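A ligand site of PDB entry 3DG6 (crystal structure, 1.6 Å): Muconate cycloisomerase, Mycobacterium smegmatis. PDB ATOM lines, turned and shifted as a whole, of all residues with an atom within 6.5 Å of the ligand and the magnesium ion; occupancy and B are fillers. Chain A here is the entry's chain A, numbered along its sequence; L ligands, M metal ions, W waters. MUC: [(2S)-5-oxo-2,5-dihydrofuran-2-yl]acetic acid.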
ATOM      1  N   LEU A  19      31.112  -6.326  21.751  1.00  0.00           N
ATOM      2  CA  LEU A  19      29.893  -6.252  22.553  1.00  0.00           C
ATOM      3  C   LEU A  19      30.100  -7.207  23.719  1.00  0.00           C
ATOM      4  O   LEU A  19      30.323  -8.408  23.526  1.00  0.00           O
ATOM      5  CB  LEU A  19      28.677  -6.698  21.736  1.00  0.00           C
ATOM      6  CG  LEU A  19      27.321  -6.535  22.443  1.00  0.00           C
ATOM      7  CD1 LEU A  19      27.007  -5.055  22.629  1.00  0.00           C
ATOM      8  CD2 LEU A  19      26.227  -7.203  21.619  1.00  0.00           C
ATOM      9  N   PHE A  21      28.788  -8.793  27.537  1.00  0.00           N
ATOM     10  CA  PHE A  21      27.616  -9.075  28.361  1.00  0.00           C
ATOM     11  C   PHE A  21      27.960 -10.152  29.390  1.00  0.00           C
ATOM     12  O   PHE A  21      29.048 -10.717  29.361  1.00  0.00           O
ATOM     13  CB  PHE A  21      26.432  -9.474  27.484  1.00  0.00           C
ATOM     14  CG  PHE A  21      26.798 -10.391  26.348  1.00  0.00           C
ATOM     15  CD1 PHE A  21      26.671 -11.765  26.484  1.00  0.00           C
ATOM     16  CD2 PHE A  21      27.311  -9.873  25.155  1.00  0.00           C
ATOM     17  CE1 PHE A  21      27.055 -12.624  25.441  1.00  0.00           C
ATOM     18  CE2 PHE A  21      27.692 -10.711  24.123  1.00  0.00           C
ATOM     19  CZ  PHE A  21      27.564 -12.086  24.259  1.00  0.00           C
ATOM     20  N   SER A  23      27.145 -13.330  29.872  1.00  0.00           N
ATOM     21  CA  SER A  23      27.470 -14.679  29.422  1.00  0.00           C
ATOM     22  C   SER A  23      28.638 -14.815  28.443  1.00  0.00           C
ATOM     23  O   SER A  23      29.069 -15.931  28.146  1.00  0.00           O
ATOM     24  CB  SER A  23      26.226 -15.327  28.824  1.00  0.00           C
ATOM     25  OG  SER A  23      25.694 -14.536  27.781  1.00  0.00           O
ATOM     26  N   ARG A  51      26.879 -19.212  18.787  1.00  0.00           N
ATOM     27  CA  ARG A  51      26.898 -18.609  20.113  1.00  0.00           C
ATOM     28  C   ARG A  51      27.083 -19.733  21.113  1.00  0.00           C
ATOM     29  O   ARG A  51      26.116 -20.238  21.701  1.00  0.00           O
ATOM     30  CB  ARG A  51      25.571 -17.871  20.356  1.00  0.00           C
ATOM     31  CG  ARG A  51      25.289 -16.759  19.334  1.00  0.00           C
ATOM     32  CD  ARG A  51      26.215 -15.571  19.557  1.00  0.00           C
ATOM     33  NE  ARG A  51      26.069 -14.519  18.548  1.00  0.00           N
ATOM     34  CZ  ARG A  51      26.910 -14.337  17.526  1.00  0.00           C
ATOM     35  NH1 ARG A  51      27.952 -15.148  17.371  1.00  0.00           N
ATOM     36  NH2 ARG A  51      26.734 -13.326  16.686  1.00  0.00           N
ATOM     37  N   PHE A  53      28.050 -19.758  24.100  1.00  0.00           N
ATOM     38  CA  PHE A  53      27.587 -19.379  25.431  1.00  0.00           C
ATOM     39  C   PHE A  53      26.068 -19.242  25.511  1.00  0.00           C
ATOM     40  O   PHE A  53      25.538 -18.830  26.543  1.00  0.00           O
ATOM     41  CB  PHE A  53      28.250 -18.059  25.844  1.00  0.00           C
ATOM     42  CG  PHE A  53      28.279 -17.034  24.749  1.00  0.00           C
ATOM     43  CD1 PHE A  53      27.099 -16.407  24.335  1.00  0.00           C
ATOM     44  CD2 PHE A  53      29.469 -16.722  24.100  1.00  0.00           C
ATOM     45  CE1 PHE A  53      27.116 -15.493  23.283  1.00  0.00           C
ATOM     46  CE2 PHE A  53      29.489 -15.799  23.049  1.00  0.00           C
ATOM     47  CZ  PHE A  53      28.312 -15.185  22.641  1.00  0.00           C
ATOM     48  N   THR A  54      25.379 -19.575  24.425  1.00  0.00           N
ATOM     49  CA  THR A  54      23.921 -19.488  24.380  1.00  0.00           C
ATOM     50  C   THR A  54      23.302 -20.814  23.943  1.00  0.00           C
ATOM     51  O   THR A  54      22.389 -21.316  24.596  1.00  0.00           O
ATOM     52  CB  THR A  54      23.461 -18.392  23.399  1.00  0.00           C
ATOM     53  OG1 THR A  54      24.019 -17.137  23.800  1.00  0.00           O
ATOM     54  CG2 THR A  54      21.932 -18.285  23.392  1.00  0.00           C
ATOM     55  N   TYR A  55      23.822 -21.379  22.851  1.00  0.00           N
ATOM     56  CA  TYR A  55      23.291 -22.645  22.327  1.00  0.00           C
ATOM     57  C   TYR A  55      24.330 -23.763  22.271  1.00  0.00           C
ATOM     58  O   TYR A  55      23.977 -24.932  22.137  1.00  0.00           O
ATOM     59  CB  TYR A  55      22.737 -22.443  20.920  1.00  0.00           C
ATOM     60  CG  TYR A  55      21.737 -21.331  20.819  1.00  0.00           C
ATOM     61  CD1 TYR A  55      20.573 -21.337  21.582  1.00  0.00           C
ATOM     62  CD2 TYR A  55      21.948 -20.257  19.952  1.00  0.00           C
ATOM     63  CE1 TYR A  55      19.646 -20.301  21.498  1.00  0.00           C
ATOM     64  CE2 TYR A  55      21.031 -19.212  19.863  1.00  0.00           C
ATOM     65  CZ  TYR A  55      19.888 -19.247  20.638  1.00  0.00           C
ATOM     66  OH  TYR A  55      18.982 -18.215  20.548  1.00  0.00           O
ATOM     67  N   MET A 134      20.721  -2.774  21.965  1.00  0.00           N
ATOM     68  CA  MET A 134      21.264  -3.412  23.162  1.00  0.00           C
ATOM     69  C   MET A 134      22.574  -2.710  23.540  1.00  0.00           C
ATOM     70  O   MET A 134      23.495  -2.640  22.730  1.00  0.00           O
ATOM     71  CB  MET A 134      21.537  -4.899  22.911  1.00  0.00           C
ATOM     72  CG  MET A 134      20.370  -5.671  22.305  1.00  0.00           C
ATOM     73  SD  MET A 134      20.586  -7.473  22.341  1.00  0.00           S
ATOM     74  CE  MET A 134      21.979  -7.688  21.214  1.00  0.00           C
ATOM     75  N   LYS A 160      17.865  -1.631  25.489  1.00  0.00           N
ATOM     76  CA  LYS A 160      17.881  -2.781  26.383  1.00  0.00           C
ATOM     77  C   LYS A 160      19.281  -2.758  26.988  1.00  0.00           C
ATOM     78  O   LYS A 160      20.266  -3.008  26.298  1.00  0.00           O
ATOM     79  CB  LYS A 160      17.654  -4.096  25.633  1.00  0.00           C
ATOM     80  CG  LYS A 160      17.665  -5.309  26.573  1.00  0.00           C
ATOM     81  CD  LYS A 160      17.173  -6.599  25.926  1.00  0.00           C
ATOM     82  CE  LYS A 160      18.254  -7.318  25.141  1.00  0.00           C
ATOM     83  NZ  LYS A 160      17.730  -8.616  24.612  1.00  0.00           N
ATOM     84  N   LYS A 162      22.374  -4.059  29.079  1.00  0.00           N
ATOM     85  CA  LYS A 162      22.972  -5.320  29.507  1.00  0.00           C
ATOM     86  C   LYS A 162      23.410  -5.139  30.946  1.00  0.00           C
ATOM     87  O   LYS A 162      24.135  -4.198  31.278  1.00  0.00           O
ATOM     88  CB  LYS A 162      24.201  -5.659  28.648  1.00  0.00           C
ATOM     89  CG  LYS A 162      23.877  -6.132  27.246  1.00  0.00           C
ATOM     90  CD  LYS A 162      23.072  -7.408  27.267  1.00  0.00           C
ATOM     91  CE  LYS A 162      22.846  -7.953  25.877  1.00  0.00           C
ATOM     92  NZ  LYS A 162      22.110  -9.234  25.935  1.00  0.00           N
ATOM     93  N   ASP A 191      18.562  -6.780  30.502  1.00  0.00           N
ATOM     94  CA  ASP A 191      18.854  -8.184  30.191  1.00  0.00           C
ATOM     95  C   ASP A 191      20.109  -8.557  30.982  1.00  0.00           C
ATOM     96  O   ASP A 191      21.182  -7.977  30.778  1.00  0.00           O
ATOM     97  CB  ASP A 191      19.127  -8.337  28.692  1.00  0.00           C
ATOM     98  CG  ASP A 191      19.250  -9.796  28.261  1.00  0.00           C
ATOM     99  OD1 ASP A 191      19.531 -10.666  29.105  1.00  0.00           O
ATOM    100  OD2 ASP A 191      19.087 -10.069  27.048  1.00  0.00           O
ATOM    101  N   ASN A 193      21.444 -11.733  31.112  1.00  0.00           N
ATOM    102  CA  ASN A 193      22.135 -12.877  30.551  1.00  0.00           C
ATOM    103  C   ASN A 193      22.598 -13.893  31.592  1.00  0.00           C
ATOM    104  O   ASN A 193      23.740 -14.373  31.543  1.00  0.00           O
ATOM    105  CB  ASN A 193      23.331 -12.435  29.696  1.00  0.00           C
ATOM    106  CG  ASN A 193      22.900 -11.821  28.384  1.00  0.00           C
ATOM    107  OD1 ASN A 193      23.071 -10.629  28.160  1.00  0.00           O
ATOM    108  ND2 ASN A 193      22.339 -12.649  27.507  1.00  0.00           N
ATOM    109  N   GLU A 217      14.758  -9.196  31.551  1.00  0.00           N
ATOM    110  CA  GLU A 217      15.094 -10.356  30.726  1.00  0.00           C
ATOM    111  C   GLU A 217      16.241 -11.199  31.290  1.00  0.00           C
ATOM    112  O   GLU A 217      17.342 -10.697  31.530  1.00  0.00           O
ATOM    113  CB  GLU A 217      15.449  -9.903  29.306  1.00  0.00           C
ATOM    114  CG  GLU A 217      15.721 -11.042  28.325  1.00  0.00           C
ATOM    115  CD  GLU A 217      15.916 -10.557  26.898  1.00  0.00           C
ATOM    116  OE1 GLU A 217      15.366  -9.498  26.559  1.00  0.00           O
ATOM    117  OE2 GLU A 217      16.604 -11.260  26.126  1.00  0.00           O
ATOM    118  N   GLU A 218      15.970 -12.488  31.497  1.00  0.00           N
ATOM    119  CA  GLU A 218      16.966 -13.444  31.984  1.00  0.00           C
ATOM    120  C   GLU A 218      17.927 -12.855  33.030  1.00  0.00           C
ATOM    121  O   GLU A 218      19.150 -12.986  32.893  1.00  0.00           O
ATOM    122  CB  GLU A 218      17.777 -13.990  30.800  1.00  0.00           C
ATOM    123  CG  GLU A 218      16.969 -14.745  29.748  1.00  0.00           C
ATOM    124  CD  GLU A 218      16.598 -16.156  30.188  1.00  0.00           C
ATOM    125  OE1 GLU A 218      16.923 -16.532  31.323  1.00  0.00           O
ATOM    126  OE2 GLU A 218      15.992 -16.891  29.375  1.00  0.00           O
ATOM    127  N   ILE A 240      11.067 -11.627  30.543  1.00  0.00           N
ATOM    128  CA  ILE A 240      11.357 -12.247  29.259  1.00  0.00           C
ATOM    129  C   ILE A 240      12.347 -13.397  29.351  1.00  0.00           C
ATOM    130  O   ILE A 240      13.449 -13.247  29.886  1.00  0.00           O
ATOM    131  CB  ILE A 240      11.925 -11.216  28.261  1.00  0.00           C
ATOM    132  CG1 ILE A 240      10.912 -10.114  27.990  1.00  0.00           C
ATOM    133  CG2 ILE A 240      12.327 -11.914  26.961  1.00  0.00           C
ATOM    134  CD1 ILE A 240      11.465  -8.967  27.150  1.00  0.00           C
ATOM    135  N   ASP A 242      14.690 -15.911  27.230  1.00  0.00           N
ATOM    136  CA  ASP A 242      15.408 -15.832  25.962  1.00  0.00           C
ATOM    137  C   ASP A 242      16.195 -17.112  25.698  1.00  0.00           C
ATOM    138  O   ASP A 242      15.688 -18.037  25.049  1.00  0.00           O
ATOM    139  CB  ASP A 242      16.335 -14.604  26.011  1.00  0.00           C
ATOM    140  CG  ASP A 242      17.183 -14.426  24.764  1.00  0.00           C
ATOM    141  OD1 ASP A 242      17.046 -15.232  23.812  1.00  0.00           O
ATOM    142  OD2 ASP A 242      17.988 -13.474  24.722  1.00  0.00           O
ATOM    143  N   GLU A 243      17.419 -17.190  26.210  1.00  0.00           N
ATOM    144  CA  GLU A 243      18.225 -18.391  25.994  1.00  0.00           C
ATOM    145  C   GLU A 243      17.599 -19.639  26.616  1.00  0.00           C
ATOM    146  O   GLU A 243      17.937 -20.764  26.241  1.00  0.00           O
ATOM    147  CB  GLU A 243      19.654 -18.199  26.526  1.00  0.00           C
ATOM    148  CG  GLU A 243      19.760 -17.683  27.947  1.00  0.00           C
ATOM    149  CD  GLU A 243      20.005 -16.183  28.002  1.00  0.00           C
ATOM    150  OE1 GLU A 243      20.896 -15.754  28.762  1.00  0.00           O
ATOM    151  OE2 GLU A 243      19.313 -15.435  27.287  1.00  0.00           O
ATOM    152  N   SER A 264      10.971 -14.082  24.287  1.00  0.00           N
ATOM    153  CA  SER A 264      11.807 -13.466  23.270  1.00  0.00           C
ATOM    154  C   SER A 264      11.746 -14.356  22.043  1.00  0.00           C
ATOM    155  O   SER A 264      11.893 -15.573  22.149  1.00  0.00           O
ATOM    156  CB  SER A 264      13.260 -13.388  23.760  1.00  0.00           C
ATOM    157  OG  SER A 264      14.168 -13.272  22.668  1.00  0.00           O
ATOM    158  N   LYS A 266      13.598 -15.012  18.512  1.00  0.00           N
ATOM    159  CA  LYS A 266      14.782 -14.678  17.729  1.00  0.00           C
ATOM    160  C   LYS A 266      14.805 -15.556  16.492  1.00  0.00           C
ATOM    161  O   LYS A 266      14.857 -16.776  16.579  1.00  0.00           O
ATOM    162  CB  LYS A 266      16.059 -14.883  18.549  1.00  0.00           C
ATOM    163  CG  LYS A 266      16.214 -13.868  19.674  1.00  0.00           C
ATOM    164  CD  LYS A 266      17.596 -13.929  20.296  1.00  0.00           C
ATOM    165  CE  LYS A 266      17.711 -12.967  21.471  1.00  0.00           C
ATOM    166  NZ  LYS A 266      19.067 -12.995  22.074  1.00  0.00           N
ATOM    167  N   GLY A 292      13.940 -10.373  19.507  1.00  0.00           N
ATOM    168  CA  GLY A 292      15.259 -10.147  20.061  1.00  0.00           C
ATOM    169  C   GLY A 292      16.394 -10.151  19.046  1.00  0.00           C
ATOM    170  O   GLY A 292      16.197 -10.434  17.870  1.00  0.00           O
ATOM    171  N   ASN A 293      17.586  -9.845  19.535  1.00  0.00           N
ATOM    172  CA  ASN A 293      18.784  -9.789  18.698  1.00  0.00           C
ATOM    173  C   ASN A 293      19.787 -10.827  19.169  1.00  0.00           C
ATOM    174  O   ASN A 293      20.074 -10.931  20.360  1.00  0.00           O
ATOM    175  CB  ASN A 293      19.391  -8.381  18.787  1.00  0.00           C
ATOM    176  CG  ASN A 293      20.415  -8.115  17.695  1.00  0.00           C
ATOM    177  OD1 ASN A 293      21.507  -8.686  17.688  1.00  0.00           O
ATOM    178  ND2 ASN A 293      20.060  -7.237  16.764  1.00  0.00           N
ATOM    179  N   GLN A 294      20.317 -11.610  18.232  1.00  0.00           N
ATOM    180  CA  GLN A 294      21.290 -12.665  18.529  1.00  0.00           C
ATOM    181  C   GLN A 294      22.690 -12.125  18.218  1.00  0.00           C
ATOM    182  O   GLN A 294      23.604 -12.902  17.924  1.00  0.00           O
ATOM    183  CB  GLN A 294      21.005 -13.880  17.639  1.00  0.00           C
ATOM    184  CG  GLN A 294      21.570 -15.184  18.157  1.00  0.00           C
ATOM    185  CD  GLN A 294      20.701 -15.796  19.244  1.00  0.00           C
ATOM    186  OE1 GLN A 294      19.642 -16.365  18.966  1.00  0.00           O
ATOM    187  NE2 GLN A 294      21.138 -15.665  20.484  1.00  0.00           N
ATOM    188  N   ILE A 295      22.837 -10.809  18.313  1.00  0.00           N
ATOM    189  CA  ILE A 295      24.087 -10.127  17.968  1.00  0.00           C
ATOM    190  C   ILE A 295      24.227 -10.439  16.480  1.00  0.00           C
ATOM    191  O   ILE A 295      25.265 -10.897  15.995  1.00  0.00           O
ATOM    192  CB  ILE A 295      25.294 -10.647  18.762  1.00  0.00           C
ATOM    193  CG1 ILE A 295      24.973 -10.640  20.262  1.00  0.00           C
ATOM    194  CG2 ILE A 295      26.503  -9.745  18.521  1.00  0.00           C
ATOM    195  CD1 ILE A 295      26.030 -11.277  21.138  1.00  0.00           C
ATOM    196  N   GLU A 320      14.723  -5.615  18.496  1.00  0.00           N
ATOM    197  CA  GLU A 320      16.157  -5.411  18.690  1.00  0.00           C
ATOM    198  C   GLU A 320      16.806  -5.607  17.316  1.00  0.00           C
ATOM    199  O   GLU A 320      17.187  -6.710  16.929  1.00  0.00           O
ATOM    200  CB  GLU A 320      16.649  -6.396  19.747  1.00  0.00           C
ATOM    201  CG  GLU A 320      16.100  -6.025  21.117  1.00  0.00           C
ATOM    202  CD  GLU A 320      16.142  -7.128  22.147  1.00  0.00           C
ATOM    203  OE1 GLU A 320      17.011  -8.021  22.042  1.00  0.00           O
ATOM    204  OE2 GLU A 320      15.303  -7.088  23.075  1.00  0.00           O
HETATM  205  C1  MUC L   1      20.343 -11.258  24.269  1.00  0.00           C
HETATM  206  O1  MUC L   1      19.183 -10.862  24.009  1.00  0.00           O
HETATM  207  O2  MUC L   1      20.656 -12.020  25.204  1.00  0.00           O
HETATM  208  C4  MUC L   1      23.483 -12.204  24.193  1.00  0.00           C
HETATM  209  C5  MUC L   1      23.794 -13.463  23.876  1.00  0.00           C
HETATM  210  C6  MUC L   1      23.164 -13.782  22.749  1.00  0.00           C
HETATM  211  O6  MUC L   1      23.444 -14.767  22.060  1.00  0.00           O
HETATM  212  O3  MUC L   1      22.164 -12.907  22.435  1.00  0.00           O
HETATM  213  C3  MUC L   1      22.646 -11.694  23.015  1.00  0.00           C
HETATM  214  C2  MUC L   1      21.486 -10.705  23.357  1.00  0.00           C
HETATM  215 MG    MG M   1      18.501 -11.693  25.882  1.00  0.00          MG
HETATM  216  O   HOH W   1      23.702 -15.950  26.295  1.00  0.00           O
HETATM  217  O   HOH W   2      18.769 -12.934  27.674  1.00  0.00           O
HETATM  218  O   HOH W   3      21.093 -14.981  25.243  1.00  0.00           O
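OD2 of Asp 191 sits close to NZ of Lys 162, 3.3 Å away.
N of Asn 193 sits at hydrogen-bond distance from O of Glu 218.
OE1 of Glu 217 is in salt-bridge range of NZ of Lys 160 (3.2 Å).
O of Gln 294 sits at hydrogen-bond distance from NE of Arg 51, at 3.0 Å.
NZ of Lys 160 sits close to OD2 of Asp 191.
The side-chain carboxylate (OD1) of Asp 191 is in hydrogen-bond range of the backbone NH (N) of Asn 193 (3.0 Å).
The side-chain amide nitrogen (ND2) of Asn 293 sits at hydrogen-bond distance from the backbone carbonyl oxygen (O) of Glu 320 (2.9 Å).
OD1 of Asn 293 is in hydrogen-bond range of N of Ile 295, 2.6 Å away.
Merely in contact with the ligand: Asn 293 (3.3 Å), Met 134 (3.5 Å), Phe 21 (3.7 Å), Ile 295 (3.8 Å), Arg 51 (3.8 Å) and Phe 53 (3.9 Å).
Hydrophobic or aromatic side chains within 4 Å of the ligand: Phe 21, Phe 53, Met 134 and Ile 295.
Of the 24 residues printed, 15 come within 4 Å of the ligand.
The nearest printed residue that does not touch the ligand is Glu 320 (4.1 Å).
The side-chain amino group (NZ) of Lys 266 lies close to an oxygen (O3) of the ligand (3.1 Å).
O1 of the ligand lies close to NZ of Lys 160, 2.7 Å away.
The side-chain amide nitrogen of Asn 193 sits close to an oxygen (O2) of the ligand (2.9 Å).
An oxygen (O6) of the ligand is in hydrogen-bond range of the side-chain hydroxyl of Thr 54, 3.0 Å away.
NE2 of Gln 294 sits at hydrogen-bond distance from O6 of the ligand (2.9 Å).
O2 of the ligand sits close to NZ of Lys 162, 3.2 Å away.
The magnesium ion is bound by OE2 of Glu 217 (2.0 Å).
OD2 of Asp 191 binds the magnesium ion, at 2.1 Å.
The magnesium ion is bound by O1 of the ligand.
The magnesium ion is bound by OD2 of Asp 242 (2.2 Å).
The magnesium ion is bound by water W2.
The magnesium ion is bound by O2 of the ligand (2.3 Å).
Water W2 lies within hydrogen-bond range of OE2 of Glu 243 (2.6 Å) and OD1 of Asp 191 (2.8 Å).
Water W3 lies within hydrogen-bond range of OE2 of Glu 243 (2.7 Å) and ND2 of Asn 193 (3.5 Å).
Water W1 lies within hydrogen-bond range of OG1 of Thr 54 (2.8 Å), OG of Ser 23 (2.9 Å) and O of Phe 53 (3.4 Å).
NZ of Lys 160 touches the magnesium ion, 3.4 Å away.
Along chain A the residues within 4 Å of the magnesium ion span positions 160 to 242.
The nearest printed residue that does not touch the magnesium ion is Lys 266 (4.1 Å).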
